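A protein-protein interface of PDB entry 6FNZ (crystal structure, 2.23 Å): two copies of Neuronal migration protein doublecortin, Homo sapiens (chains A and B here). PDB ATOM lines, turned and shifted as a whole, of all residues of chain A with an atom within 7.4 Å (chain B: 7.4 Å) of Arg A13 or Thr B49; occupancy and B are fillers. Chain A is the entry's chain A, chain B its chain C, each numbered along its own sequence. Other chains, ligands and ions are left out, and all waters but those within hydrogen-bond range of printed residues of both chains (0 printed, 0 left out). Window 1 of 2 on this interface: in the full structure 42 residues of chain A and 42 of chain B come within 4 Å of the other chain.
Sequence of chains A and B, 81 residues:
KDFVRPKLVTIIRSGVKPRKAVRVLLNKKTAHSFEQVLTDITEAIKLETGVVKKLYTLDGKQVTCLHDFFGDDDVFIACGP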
ATOM      1  N   ILE A  11      24.974 -12.554  33.039  1.00  0.00           N
ATOM      2  CA  ILE A  11      24.338 -11.326  33.515  1.00  0.00           C
ATOM      3  C   ILE A  11      22.826 -11.473  33.404  1.00  0.00           C
ATOM      4  O   ILE A  11      22.306 -11.818  32.336  1.00  0.00           O
ATOM      5  CB  ILE A  11      24.819 -10.088  32.731  1.00  0.00           C
ATOM      6  CG1 ILE A  11      26.330  -9.883  32.888  1.00  0.00           C
ATOM      7  CG2 ILE A  11      24.092  -8.865  33.236  1.00  0.00           C
ATOM      8  CD1 ILE A  11      26.747  -9.470  34.319  1.00  0.00           C
ATOM      9  N   ILE A  12      22.119 -11.187  34.490  1.00  0.00           N
ATOM     10  CA  ILE A  12      20.667 -11.195  34.503  1.00  0.00           C
ATOM     11  C   ILE A  12      20.184  -9.766  34.677  1.00  0.00           C
ATOM     12  O   ILE A  12      20.555  -9.089  35.641  1.00  0.00           O
ATOM     13  CB  ILE A  12      20.103 -12.088  35.614  1.00  0.00           C
ATOM     14  CG1 ILE A  12      20.433 -13.539  35.321  1.00  0.00           C
ATOM     15  CG2 ILE A  12      18.588 -11.910  35.702  1.00  0.00           C
ATOM     16  CD1 ILE A  12      20.140 -14.386  36.496  1.00  0.00           C
ATOM     17  N   ARG A  13      19.348  -9.315  33.754  1.00  0.00           N
ATOM     18  CA  ARG A  13      18.863  -7.950  33.797  1.00  0.00           C
ATOM     19  C   ARG A  13      17.754  -7.853  34.827  1.00  0.00           C
ATOM     20  O   ARG A  13      16.781  -8.626  34.789  1.00  0.00           O
ATOM     21  CB  ARG A  13      18.401  -7.537  32.415  1.00  0.00           C
ATOM     22  CG  ARG A  13      19.537  -7.749  31.418  1.00  0.00           C
ATOM     23  CD  ARG A  13      19.058  -7.249  30.058  1.00  0.00           C
ATOM     24  NE  ARG A  13      18.628  -5.873  30.217  1.00  0.00           N
ATOM     25  CZ  ARG A  13      17.902  -5.215  29.318  1.00  0.00           C
ATOM     26  NH1 ARG A  13      17.550  -5.806  28.186  1.00  0.00           N
ATOM     27  NH2 ARG A  13      17.540  -3.963  29.544  1.00  0.00           N
ATOM     28  N   SER A  14      17.927  -6.942  35.779  1.00  0.00           N
ATOM     29  CA  SER A  14      16.934  -6.796  36.831  1.00  0.00           C
ATOM     30  C   SER A  14      15.593  -6.441  36.218  1.00  0.00           C
ATOM     31  O   SER A  14      15.498  -5.524  35.394  1.00  0.00           O
ATOM     32  CB  SER A  14      17.344  -5.717  37.819  1.00  0.00           C
ATOM     33  OG  SER A  14      16.434  -5.698  38.896  1.00  0.00           O
ATOM     34  N   GLY A  15      14.570  -7.197  36.603  1.00  0.00           N
ATOM     35  CA  GLY A  15      13.198  -6.924  36.230  1.00  0.00           C
ATOM     36  C   GLY A  15      12.800  -7.315  34.823  1.00  0.00           C
ATOM     37  O   GLY A  15      11.613  -7.240  34.496  1.00  0.00           O
ATOM     38  N   VAL A  16      13.731  -7.742  33.975  1.00  0.00           N
ATOM     39  CA  VAL A  16      13.450  -7.872  32.548  1.00  0.00           C
ATOM     40  C   VAL A  16      12.969  -9.284  32.228  1.00  0.00           C
ATOM     41  O   VAL A  16      13.583 -10.282  32.628  1.00  0.00           O
ATOM     42  CB  VAL A  16      14.679  -7.496  31.712  1.00  0.00           C
ATOM     43  CG1 VAL A  16      14.507  -7.970  30.263  1.00  0.00           C
ATOM     44  CG2 VAL A  16      14.883  -5.970  31.771  1.00  0.00           C
ATOM     45  N   LYS A  17      11.846  -9.361  31.522  1.00  0.00           N
ATOM     46  CA  LYS A  17      11.300 -10.626  31.075  1.00  0.00           C
ATOM     47  C   LYS A  17      11.148 -10.590  29.562  1.00  0.00           C
ATOM     48  O   LYS A  17      10.898  -9.528  28.994  1.00  0.00           O
ATOM     49  CB  LYS A  17       9.947 -10.931  31.729  1.00  0.00           C
ATOM     50  CG  LYS A  17      10.023 -11.230  33.228  1.00  0.00           C
ATOM     51  CD  LYS A  17       8.639 -11.113  33.833  1.00  0.00           C
ATOM     52  CE  LYS A  17       8.463 -11.994  35.044  1.00  0.00           C
ATOM     53  NZ  LYS A  17       7.029 -12.337  35.330  1.00  0.00           N
ATOM     54  N   PRO A  18      11.334 -11.721  28.874  1.00  0.00           N
ATOM     55  CA  PRO A  18      11.696 -13.058  29.376  1.00  0.00           C
ATOM     56  C   PRO A  18      13.058 -13.092  30.040  1.00  0.00           C
ATOM     57  O   PRO A  18      13.829 -12.160  29.871  1.00  0.00           O
ATOM     58  CB  PRO A  18      11.693 -13.925  28.119  1.00  0.00           C
ATOM     59  CG  PRO A  18      11.851 -12.944  26.974  1.00  0.00           C
ATOM     60  CD  PRO A  18      11.171 -11.696  27.412  1.00  0.00           C
ATOM     61  N   ARG A  19      13.310 -14.147  30.812  1.00  0.00           N
ATOM     62  CA  ARG A  19      14.562 -14.328  31.535  1.00  0.00           C
ATOM     63  C   ARG A  19      15.605 -14.903  30.589  1.00  0.00           C
ATOM     64  O   ARG A  19      15.629 -16.108  30.326  1.00  0.00           O
ATOM     65  CB  ARG A  19      14.332 -15.244  32.729  1.00  0.00           C
ATOM     66  CG  ARG A  19      13.280 -14.698  33.665  1.00  0.00           C
ATOM     67  CD  ARG A  19      13.775 -13.375  34.204  1.00  0.00           C
ATOM     68  NE  ARG A  19      13.013 -12.915  35.354  1.00  0.00           N
ATOM     69  CZ  ARG A  19      13.424 -11.931  36.149  1.00  0.00           C
ATOM     70  NH1 ARG A  19      14.586 -11.322  35.909  1.00  0.00           N
ATOM     71  NH2 ARG A  19      12.672 -11.552  37.173  1.00  0.00           N
ATOM     72  N   LYS A  20      16.477 -14.050  30.065  1.00  0.00           N
ATOM     73  CA  LYS A  20      17.520 -14.511  29.158  1.00  0.00           C
ATOM     74  C   LYS A  20      18.882 -14.085  29.678  1.00  0.00           C
ATOM     75  O   LYS A  20      19.105 -12.903  29.960  1.00  0.00           O
ATOM     76  CB  LYS A  20      17.312 -13.975  27.744  1.00  0.00           C
ATOM     77  CG  LYS A  20      16.058 -14.494  27.068  1.00  0.00           C
ATOM     78  CD  LYS A  20      16.192 -14.367  25.565  1.00  0.00           C
ATOM     79  CE  LYS A  20      15.123 -15.185  24.874  1.00  0.00           C
ATOM     80  NZ  LYS A  20      14.624 -14.513  23.640  1.00  0.00           N
ATOM     81  N   ALA A  21      19.789 -15.050  29.792  1.00  0.00           N
ATOM     82  CA  ALA A  21      21.130 -14.773  30.276  1.00  0.00           C
ATOM     83  C   ALA A  21      21.918 -14.010  29.215  1.00  0.00           C
ATOM     84  O   ALA A  21      21.839 -14.318  28.024  1.00  0.00           O
ATOM     85  CB  ALA A  21      21.836 -16.093  30.619  1.00  0.00           C
ATOM     86  N   VAL A  22      22.678 -13.008  29.642  1.00  0.00           N
ATOM     87  CA  VAL A  22      23.629 -12.328  28.767  1.00  0.00           C
ATOM     88  C   VAL A  22      25.034 -12.722  29.225  1.00  0.00           C
ATOM     89  O   VAL A  22      25.403 -12.510  30.388  1.00  0.00           O
ATOM     90  CB  VAL A  22      23.421 -10.805  28.779  1.00  0.00           C
ATOM     91  CG1 VAL A  22      24.470 -10.131  27.932  1.00  0.00           C
ATOM     92  CG2 VAL A  22      21.975 -10.429  28.248  1.00  0.00           C
ATOM     93  N   ILE A  41      29.492  -4.813  29.574  1.00  0.00           N
ATOM     94  CA  ILE A  41      28.232  -5.494  29.852  1.00  0.00           C
ATOM     95  C   ILE A  41      27.094  -4.775  29.143  1.00  0.00           C
ATOM     96  O   ILE A  41      26.204  -5.396  28.546  1.00  0.00           O
ATOM     97  CB  ILE A  41      27.988  -5.576  31.368  1.00  0.00           C
ATOM     98  CG1 ILE A  41      29.009  -6.520  32.031  1.00  0.00           C
ATOM     99  CG2 ILE A  41      26.599  -6.113  31.626  1.00  0.00           C
ATOM    100  CD1 ILE A  41      29.045  -6.395  33.549  1.00  0.00           C
ATOM    101  N   THR A  42      27.137  -3.449  29.162  1.00  0.00           N
ATOM    102  CA  THR A  42      26.123  -2.669  28.485  1.00  0.00           C
ATOM    103  C   THR A  42      26.083  -3.018  27.008  1.00  0.00           C
ATOM    104  O   THR A  42      25.009  -3.299  26.460  1.00  0.00           O
ATOM    105  CB  THR A  42      26.386  -1.187  28.698  1.00  0.00           C
ATOM    106  OG1 THR A  42      26.377  -0.909  30.113  1.00  0.00           O
ATOM    107  CG2 THR A  42      25.310  -0.365  27.973  1.00  0.00           C
ATOM    108  N   ILE A  45      24.513  -6.393  26.340  1.00  0.00           N
ATOM    109  CA  ILE A  45      23.057  -6.344  26.452  1.00  0.00           C
ATOM    110  C   ILE A  45      22.457  -5.756  25.188  1.00  0.00           C
ATOM    111  O   ILE A  45      21.517  -6.312  24.612  1.00  0.00           O
ATOM    112  CB  ILE A  45      22.636  -5.545  27.699  1.00  0.00           C
ATOM    113  CG1 ILE A  45      22.989  -6.316  28.976  1.00  0.00           C
ATOM    114  CG2 ILE A  45      21.119  -5.230  27.650  1.00  0.00           C
ATOM    115  CD1 ILE A  45      22.677  -5.504  30.262  1.00  0.00           C
ATOM    116  N   LYS A  46      23.017  -4.635  24.717  1.00  0.00           N
ATOM    117  CA  LYS A  46      22.505  -4.017  23.498  1.00  0.00           C
ATOM    118  C   LYS A  46      22.600  -4.971  22.315  1.00  0.00           C
ATOM    119  O   LYS A  46      21.715  -4.995  21.449  1.00  0.00           O
ATOM    120  CB  LYS A  46      23.257  -2.712  23.204  1.00  0.00           C
ATOM    121  CG  LYS A  46      22.967  -1.628  24.206  1.00  0.00           C
ATOM    122  CD  LYS A  46      23.507  -0.250  23.825  1.00  0.00           C
ATOM    123  CE  LYS A  46      23.060   0.756  24.885  1.00  0.00           C
ATOM    124  NZ  LYS A  46      23.385   2.167  24.563  1.00  0.00           N
ATOM    125  N   LEU A  47      23.669  -5.763  22.260  1.00  0.00           N
ATOM    126  CA  LEU A  47      23.850  -6.666  21.135  1.00  0.00           C
ATOM    127  C   LEU A  47      22.793  -7.763  21.117  1.00  0.00           C
ATOM    128  O   LEU A  47      22.393  -8.214  20.041  1.00  0.00           O
ATOM    129  CB  LEU A  47      25.253  -7.260  21.198  1.00  0.00           C
ATOM    130  CG  LEU A  47      25.802  -7.804  19.890  1.00  0.00           C
ATOM    131  CD1 LEU A  47      25.871  -6.691  18.853  1.00  0.00           C
ATOM    132  CD2 LEU A  47      27.171  -8.421  20.122  1.00  0.00           C
ATOM    133  N   GLU A  48      22.318  -8.196  22.288  1.00  0.00           N
ATOM    134  CA  GLU A  48      21.317  -9.254  22.345  1.00  0.00           C
ATOM    135  C   GLU A  48      19.931  -8.774  21.948  1.00  0.00           C
ATOM    136  O   GLU A  48      19.025  -9.606  21.833  1.00  0.00           O
ATOM    137  CB  GLU A  48      21.259  -9.878  23.746  1.00  0.00           C
ATOM    138  CG  GLU A  48      22.454 -10.784  24.047  1.00  0.00           C
ATOM    139  CD  GLU A  48      22.696 -11.829  22.964  1.00  0.00           C
ATOM    140  OE1 GLU A  48      21.771 -12.623  22.684  1.00  0.00           O
ATOM    141  OE2 GLU A  48      23.805 -11.851  22.384  1.00  0.00           O
ATOM    142  N   THR A  49      19.745  -7.467  21.763  1.00  0.00           N
ATOM    143  CA  THR A  49      18.508  -6.923  21.224  1.00  0.00           C
ATOM    144  C   THR A  49      18.274  -7.456  19.814  1.00  0.00           C
ATOM    145  O   THR A  49      19.044  -7.168  18.890  1.00  0.00           O
ATOM    146  CB  THR A  49      18.557  -5.388  21.221  1.00  0.00           C
ATOM    147  OG1 THR A  49      18.286  -4.889  22.533  1.00  0.00           O
ATOM    148  CG2 THR A  49      17.545  -4.817  20.240  1.00  0.00           C
ATOM    149  N   ARG B  13       7.375  -3.385  22.350  1.00  0.00           N
ATOM    150  CA  ARG B  13       8.155  -4.573  22.031  1.00  0.00           C
ATOM    151  C   ARG B  13       7.399  -5.808  22.474  1.00  0.00           C
ATOM    152  O   ARG B  13       6.963  -5.908  23.629  1.00  0.00           O
ATOM    153  CB  ARG B  13       9.517  -4.521  22.692  1.00  0.00           C
ATOM    154  CG  ARG B  13      10.338  -3.330  22.225  1.00  0.00           C
ATOM    155  CD  ARG B  13      11.664  -3.340  22.937  1.00  0.00           C
ATOM    156  NE  ARG B  13      12.377  -4.570  22.644  1.00  0.00           N
ATOM    157  CZ  ARG B  13      13.377  -5.040  23.391  1.00  0.00           C
ATOM    158  NH1 ARG B  13      13.772  -4.370  24.481  1.00  0.00           N
ATOM    159  NH2 ARG B  13      13.968  -6.186  23.056  1.00  0.00           N
ATOM    160  N   VAL B  16       7.951  -8.305  25.840  1.00  0.00           N
ATOM    161  CA  VAL B  16       9.009  -7.760  26.681  1.00  0.00           C
ATOM    162  C   VAL B  16       8.379  -7.080  27.890  1.00  0.00           C
ATOM    163  O   VAL B  16       7.429  -6.291  27.754  1.00  0.00           O
ATOM    164  CB  VAL B  16       9.897  -6.784  25.894  1.00  0.00           C
ATOM    165  CG1 VAL B  16      10.811  -6.022  26.856  1.00  0.00           C
ATOM    166  CG2 VAL B  16      10.713  -7.542  24.869  1.00  0.00           C
ATOM    167  N   LYS B  17       8.897  -7.398  29.073  1.00  0.00           N
ATOM    168  CA  LYS B  17       8.492  -6.732  30.298  1.00  0.00           C
ATOM    169  C   LYS B  17       9.715  -6.156  30.989  1.00  0.00           C
ATOM    170  O   LYS B  17      10.797  -6.748  30.933  1.00  0.00           O
ATOM    171  CB  LYS B  17       7.766  -7.694  31.247  1.00  0.00           C
ATOM    172  CG  LYS B  17       6.396  -8.117  30.777  1.00  0.00           C
ATOM    173  CD  LYS B  17       5.843  -9.181  31.691  1.00  0.00           C
ATOM    174  CE  LYS B  17       4.566  -9.777  31.127  1.00  0.00           C
ATOM    175  NZ  LYS B  17       4.015 -10.823  32.034  1.00  0.00           N
ATOM    176  N   PRO B  18       9.579  -4.998  31.650  1.00  0.00           N
ATOM    177  CA  PRO B  18       8.342  -4.233  31.832  1.00  0.00           C
ATOM    178  C   PRO B  18       7.871  -3.563  30.563  1.00  0.00           C
ATOM    179  O   PRO B  18       8.596  -3.554  29.574  1.00  0.00           O
ATOM    180  CB  PRO B  18       8.729  -3.186  32.872  1.00  0.00           C
ATOM    181  CG  PRO B  18      10.173  -2.947  32.610  1.00  0.00           C
ATOM    182  CD  PRO B  18      10.736  -4.297  32.228  1.00  0.00           C
ATOM    183  N   VAL B  22       8.697   2.764  23.488  1.00  0.00           N
ATOM    184  CA  VAL B  22       9.851   3.305  22.778  1.00  0.00           C
ATOM    185  C   VAL B  22       9.331   4.256  21.712  1.00  0.00           C
ATOM    186  O   VAL B  22       8.545   3.855  20.840  1.00  0.00           O
ATOM    187  CB  VAL B  22      10.712   2.194  22.155  1.00  0.00           C
ATOM    188  CG1 VAL B  22      11.811   2.803  21.359  1.00  0.00           C
ATOM    189  CG2 VAL B  22      11.280   1.224  23.266  1.00  0.00           C
ATOM    190  N   GLU B  43      17.476   0.678  16.209  1.00  0.00           N
ATOM    191  CA  GLU B  43      18.417   1.562  16.894  1.00  0.00           C
ATOM    192  C   GLU B  43      17.755   2.269  18.073  1.00  0.00           C
ATOM    193  O   GLU B  43      18.357   2.390  19.150  1.00  0.00           O
ATOM    194  CB  GLU B  43      19.010   2.571  15.913  1.00  0.00           C
ATOM    195  CG  GLU B  43      19.991   1.951  14.913  1.00  0.00           C
ATOM    196  CD  GLU B  43      20.903   0.894  15.537  1.00  0.00           C
ATOM    197  OE1 GLU B  43      20.712  -0.306  15.245  1.00  0.00           O
ATOM    198  OE2 GLU B  43      21.800   1.258  16.326  1.00  0.00           O
ATOM    199  N   ALA B  44      16.502   2.714  17.908  1.00  0.00           N
ATOM    200  CA  ALA B  44      15.821   3.383  19.018  1.00  0.00           C
ATOM    201  C   ALA B  44      15.674   2.460  20.215  1.00  0.00           C
ATOM    202  O   ALA B  44      15.795   2.894  21.368  1.00  0.00           O
ATOM    203  CB  ALA B  44      14.440   3.889  18.595  1.00  0.00           C
ATOM    204  N   ILE B  45      15.388   1.183  19.960  1.00  0.00           N
ATOM    205  CA  ILE B  45      15.240   0.219  21.047  1.00  0.00           C
ATOM    206  C   ILE B  45      16.577   0.018  21.768  1.00  0.00           C
ATOM    207  O   ILE B  45      16.655   0.113  22.995  1.00  0.00           O
ATOM    208  CB  ILE B  45      14.665  -1.100  20.501  1.00  0.00           C
ATOM    209  CG1 ILE B  45      13.196  -0.896  20.126  1.00  0.00           C
ATOM    210  CG2 ILE B  45      14.848  -2.239  21.495  1.00  0.00           C
ATOM    211  CD1 ILE B  45      12.592  -2.087  19.439  1.00  0.00           C
ATOM    212  N   LYS B  46      17.661  -0.200  21.014  1.00  0.00           N
ATOM    213  CA  LYS B  46      18.955  -0.399  21.663  1.00  0.00           C
ATOM    214  C   LYS B  46      19.351   0.816  22.492  1.00  0.00           C
ATOM    215  O   LYS B  46      19.970   0.668  23.553  1.00  0.00           O
ATOM    216  CB  LYS B  46      20.042  -0.715  20.629  1.00  0.00           C
ATOM    217  CG  LYS B  46      19.716  -1.862  19.680  1.00  0.00           C
ATOM    218  CD  LYS B  46      20.968  -2.420  18.977  1.00  0.00           C
ATOM    219  CE  LYS B  46      20.611  -3.662  18.153  1.00  0.00           C
ATOM    220  NZ  LYS B  46      21.734  -4.608  17.885  1.00  0.00           N
ATOM    221  N   LEU B  47      18.980   2.020  22.049  1.00  0.00           N
ATOM    222  CA  LEU B  47      19.371   3.213  22.795  1.00  0.00           C
ATOM    223  C   LEU B  47      18.648   3.292  24.130  1.00  0.00           C
ATOM    224  O   LEU B  47      19.255   3.630  25.149  1.00  0.00           O
ATOM    225  CB  LEU B  47      19.105   4.462  21.957  1.00  0.00           C
ATOM    226  CG  LEU B  47      19.436   5.809  22.603  1.00  0.00           C
ATOM    227  CD1 LEU B  47      20.746   5.776  23.392  1.00  0.00           C
ATOM    228  CD2 LEU B  47      19.513   6.849  21.515  1.00  0.00           C
ATOM    229  N   GLU B  48      17.354   2.966  24.152  1.00  0.00           N
ATOM    230  CA  GLU B  48      16.580   3.058  25.386  1.00  0.00           C
ATOM    231  C   GLU B  48      16.922   1.959  26.379  1.00  0.00           C
ATOM    232  O   GLU B  48      16.517   2.050  27.541  1.00  0.00           O
ATOM    233  CB  GLU B  48      15.084   3.023  25.075  1.00  0.00           C
ATOM    234  CG  GLU B  48      14.651   4.006  23.986  1.00  0.00           C
ATOM    235  CD  GLU B  48      14.778   5.473  24.384  1.00  0.00           C
ATOM    236  OE1 GLU B  48      15.024   5.747  25.585  1.00  0.00           O
ATOM    237  OE2 GLU B  48      14.621   6.342  23.485  1.00  0.00           O
ATOM    238  N   THR B  49      17.611   0.907  25.945  1.00  0.00           N
ATOM    239  CA  THR B  49      18.229  -0.009  26.883  1.00  0.00           C
ATOM    240  C   THR B  49      19.197   0.790  27.742  1.00  0.00           C
ATOM    241  O   THR B  49      20.172   1.353  27.234  1.00  0.00           O
ATOM    242  CB  THR B  49      18.929  -1.135  26.126  1.00  0.00           C
ATOM    243  OG1 THR B  49      17.939  -1.965  25.506  1.00  0.00           O
ATOM    244  CG2 THR B  49      19.739  -1.942  27.047  1.00  0.00           C
ATOM    245  N   GLY B  50      18.917   0.891  29.034  1.00  0.00           N
ATOM    246  CA  GLY B  50      19.727   1.750  29.876  1.00  0.00           C
ATOM    247  C   GLY B  50      21.158   1.259  29.977  1.00  0.00           C
ATOM    248  O   GLY B  50      21.440   0.067  29.875  1.00  0.00           O
ATOM    249  N   VAL B  51      22.078   2.199  30.175  1.00  0.00           N
ATOM    250  CA  VAL B  51      23.452   1.827  30.471  1.00  0.00           C
ATOM    251  C   VAL B  51      23.516   1.212  31.864  1.00  0.00           C
ATOM    252  O   VAL B  51      22.805   1.633  32.786  1.00  0.00           O
ATOM    253  CB  VAL B  51      24.372   3.050  30.325  1.00  0.00           C
ATOM    254  CG1 VAL B  51      25.808   2.691  30.663  1.00  0.00           C
ATOM    255  CG2 VAL B  51      24.294   3.546  28.892  1.00  0.00           C
ATOM    256  N   VAL B  52      24.352   0.186  32.017  1.00  0.00           N
ATOM    257  CA  VAL B  52      24.442  -0.520  33.289  1.00  0.00           C
ATOM    258  C   VAL B  52      25.209   0.351  34.271  1.00  0.00           C
ATOM    259  O   VAL B  52      26.339   0.761  33.995  1.00  0.00           O
ATOM    260  CB  VAL B  52      25.103  -1.889  33.106  1.00  0.00           C
ATOM    261  CG1 VAL B  52      25.390  -2.513  34.473  1.00  0.00           C
ATOM    262  CG2 VAL B  52      24.194  -2.789  32.292  1.00  0.00           C
ATOM    263  N   PHE B  76      25.698 -12.470  37.931  1.00  0.00           N
ATOM    264  CA  PHE B  76      25.368 -11.187  38.552  1.00  0.00           C
ATOM    265  C   PHE B  76      24.072 -10.621  37.976  1.00  0.00           C
ATOM    266  O   PHE B  76      23.607 -11.006  36.895  1.00  0.00           O
ATOM    267  CB  PHE B  76      26.474 -10.138  38.354  1.00  0.00           C
ATOM    268  CG  PHE B  76      27.831 -10.584  38.795  1.00  0.00           C
ATOM    269  CD1 PHE B  76      28.233 -10.444  40.115  1.00  0.00           C
ATOM    270  CD2 PHE B  76      28.718 -11.125  37.890  1.00  0.00           C
ATOM    271  CE1 PHE B  76      29.497 -10.862  40.518  1.00  0.00           C
ATOM    272  CE2 PHE B  76      29.986 -11.541  38.291  1.00  0.00           C
ATOM    273  CZ  PHE B  76      30.373 -11.405  39.599  1.00  0.00           C
ATOM    274  N   ILE B  77      23.508  -9.668  38.710  1.00  0.00           N
ATOM    275  CA  ILE B  77      22.327  -8.933  38.290  1.00  0.00           C
ATOM    276  C   ILE B  77      22.742  -7.510  37.937  1.00  0.00           C
ATOM    277  O   ILE B  77      23.443  -6.850  38.718  1.00  0.00           O
ATOM    278  CB  ILE B  77      21.260  -8.947  39.391  1.00  0.00           C
ATOM    279  CG1 ILE B  77      20.930 -10.393  39.746  1.00  0.00           C
ATOM    280  CG2 ILE B  77      20.017  -8.172  38.956  1.00  0.00           C
ATOM    281  CD1 ILE B  77      20.212 -10.521  41.042  1.00  0.00           C
ATOM    282  N   ALA B  78      22.314  -7.046  36.760  1.00  0.00           N
ATOM    283  CA  ALA B  78      22.538  -5.674  36.297  1.00  0.00           C
ATOM    284  C   ALA B  78      21.363  -4.777  36.641  1.00  0.00           C
ATOM    285  O   ALA B  78      20.202  -5.173  36.503  1.00  0.00           O
ATOM    286  CB  ALA B  78      22.746  -5.627  34.782  1.00  0.00           C
ATOM    287  N   CYS B  79      21.670  -3.554  37.069  1.00  0.00           N
ATOM    288  CA  CYS B  79      20.666  -2.506  37.206  1.00  0.00           C
ATOM    289  C   CYS B  79      21.064  -1.282  36.385  1.00  0.00           C
ATOM    290  O   CYS B  79      22.247  -0.925  36.305  1.00  0.00           O
ATOM    291  CB  CYS B  79      20.469  -2.128  38.677  1.00  0.00           C
ATOM    292  SG  CYS B  79      19.919  -3.542  39.687  1.00  0.00           S
ATOM    293  N   PRO B  81      19.713   2.952  35.594  1.00  0.00           N
ATOM    294  CA  PRO B  81      19.355   4.099  36.443  1.00  0.00           C
ATOM    295  C   PRO B  81      18.334   3.747  37.531  1.00  0.00           C
ATOM    296  O   PRO B  81      18.481   4.161  38.685  1.00  0.00           O
ATOM    297  CB  PRO B  81      18.747   5.095  35.451  1.00  0.00           C
ATOM    298  CG  PRO B  81      19.233   4.683  34.095  1.00  0.00           C
ATOM    299  CD  PRO B  81      19.893   3.340  34.184  1.00  0.00           C
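The backbone NH (N) of Ile A12 is in hydrogen-bond range of the backbone carbonyl oxygen (O) of Phe B76. The backbone carbonyl oxygen (O) of Ile A12 is in hydrogen-bond range of the backbone NH (N) of Ala B78 (2.9 Å). N of Ser A14 lies within hydrogen-bond range of O of Ala B78 (3.0 Å). The backbone NH (N) of Lys A17 lies within hydrogen-bond range of the backbone carbonyl oxygen (O) of Lys B17 (2.9 Å). The side-chain hydroxyl (OG1) of Thr A42 is in hydrogen-bond range of the backbone NH (N) of Val B52.
N of Ile A11 sits at hydrogen-bond distance from O of Val A22 (2.7 Å).
Among the printed residues, pairs that only touch across the chains: Ile A12 with Ile B77, Val A16 with Lys B17, Lys A46 with Lys B46, Lys A17 with Val B16, Ile A11 with Phe B76, Ile A45 with Thr B49, Thr A42 with Val B51, Gly A15 with Lys B17, Thr A49 with Lys B46, Ile A45 with Val B52, Lys A46 with Thr B49, Ser A14 with Ile B77, Gly A15 with Pro B18, Ile A11 with Ala B78, Ser A14 with Cys B79, Arg A13 with Thr B49, Thr A49 with Ile B45 and Arg A13 with Ala B78.
Printed residues of chain B within 4 Å of Arg A13: Thr B49 and Ala B78. Printed residues of chain B within 4 Å of Val A16: Lys B17. Val A22 touches none of the printed residues of chain B. Glu A48 touches none of the printed residues of chain B. Printed residues of chain A within 4 Å of Val B16: Lys A17. Of the printed residues of chain A, Ile B45 touches Thr A49. No residue of chain A comes within 4 Å of Gly B50. The nearest printed residue of chain B that does not touch Arg A13 is Ile B77 (4.7 Å). The nearest residue of chain A that does not touch Thr B49 is Thr A49 (4.2 Å). The nearest printed residue of chain A that does not touch Ile B45 is Lys A46 (6.7 Å).
Of the 19 printed residues of chain A, 11 touch a printed residue of chain B. Of the 20 printed residues of chain B, 12 touch a printed residue of chain A. Hydrophobic or aromatic side chains of chain B that line the printed part of chain A: Pro B18, Ile B45, Val B51, Val B52, Ile B77 and Ala B78. Along chain B the printed residues that touch a printed residue of chain A span positions 16 to 79. Among the printed residues, 23 pairs touch across the chains.
Arg A13 touches Thr B49, but with the chains exchanged Thr A49 does not touch Arg B13 (4.5 Å). Ile A45 touches Thr B49, and with the chains exchanged Thr A49 touches Ile B45. Lys B46 touches its own counterpart, Lys A46. Lys A46 touches Thr B49, and with the chains exchanged Thr A49 touches Lys B46. Positions printed for both chains: 13, 16, 17, 18, 22, 45, 46, 47, 48 and 49. Of the 23 pairs that touch across the chains among the printed residues, 8 have their exchanged pair printed and touching as well.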
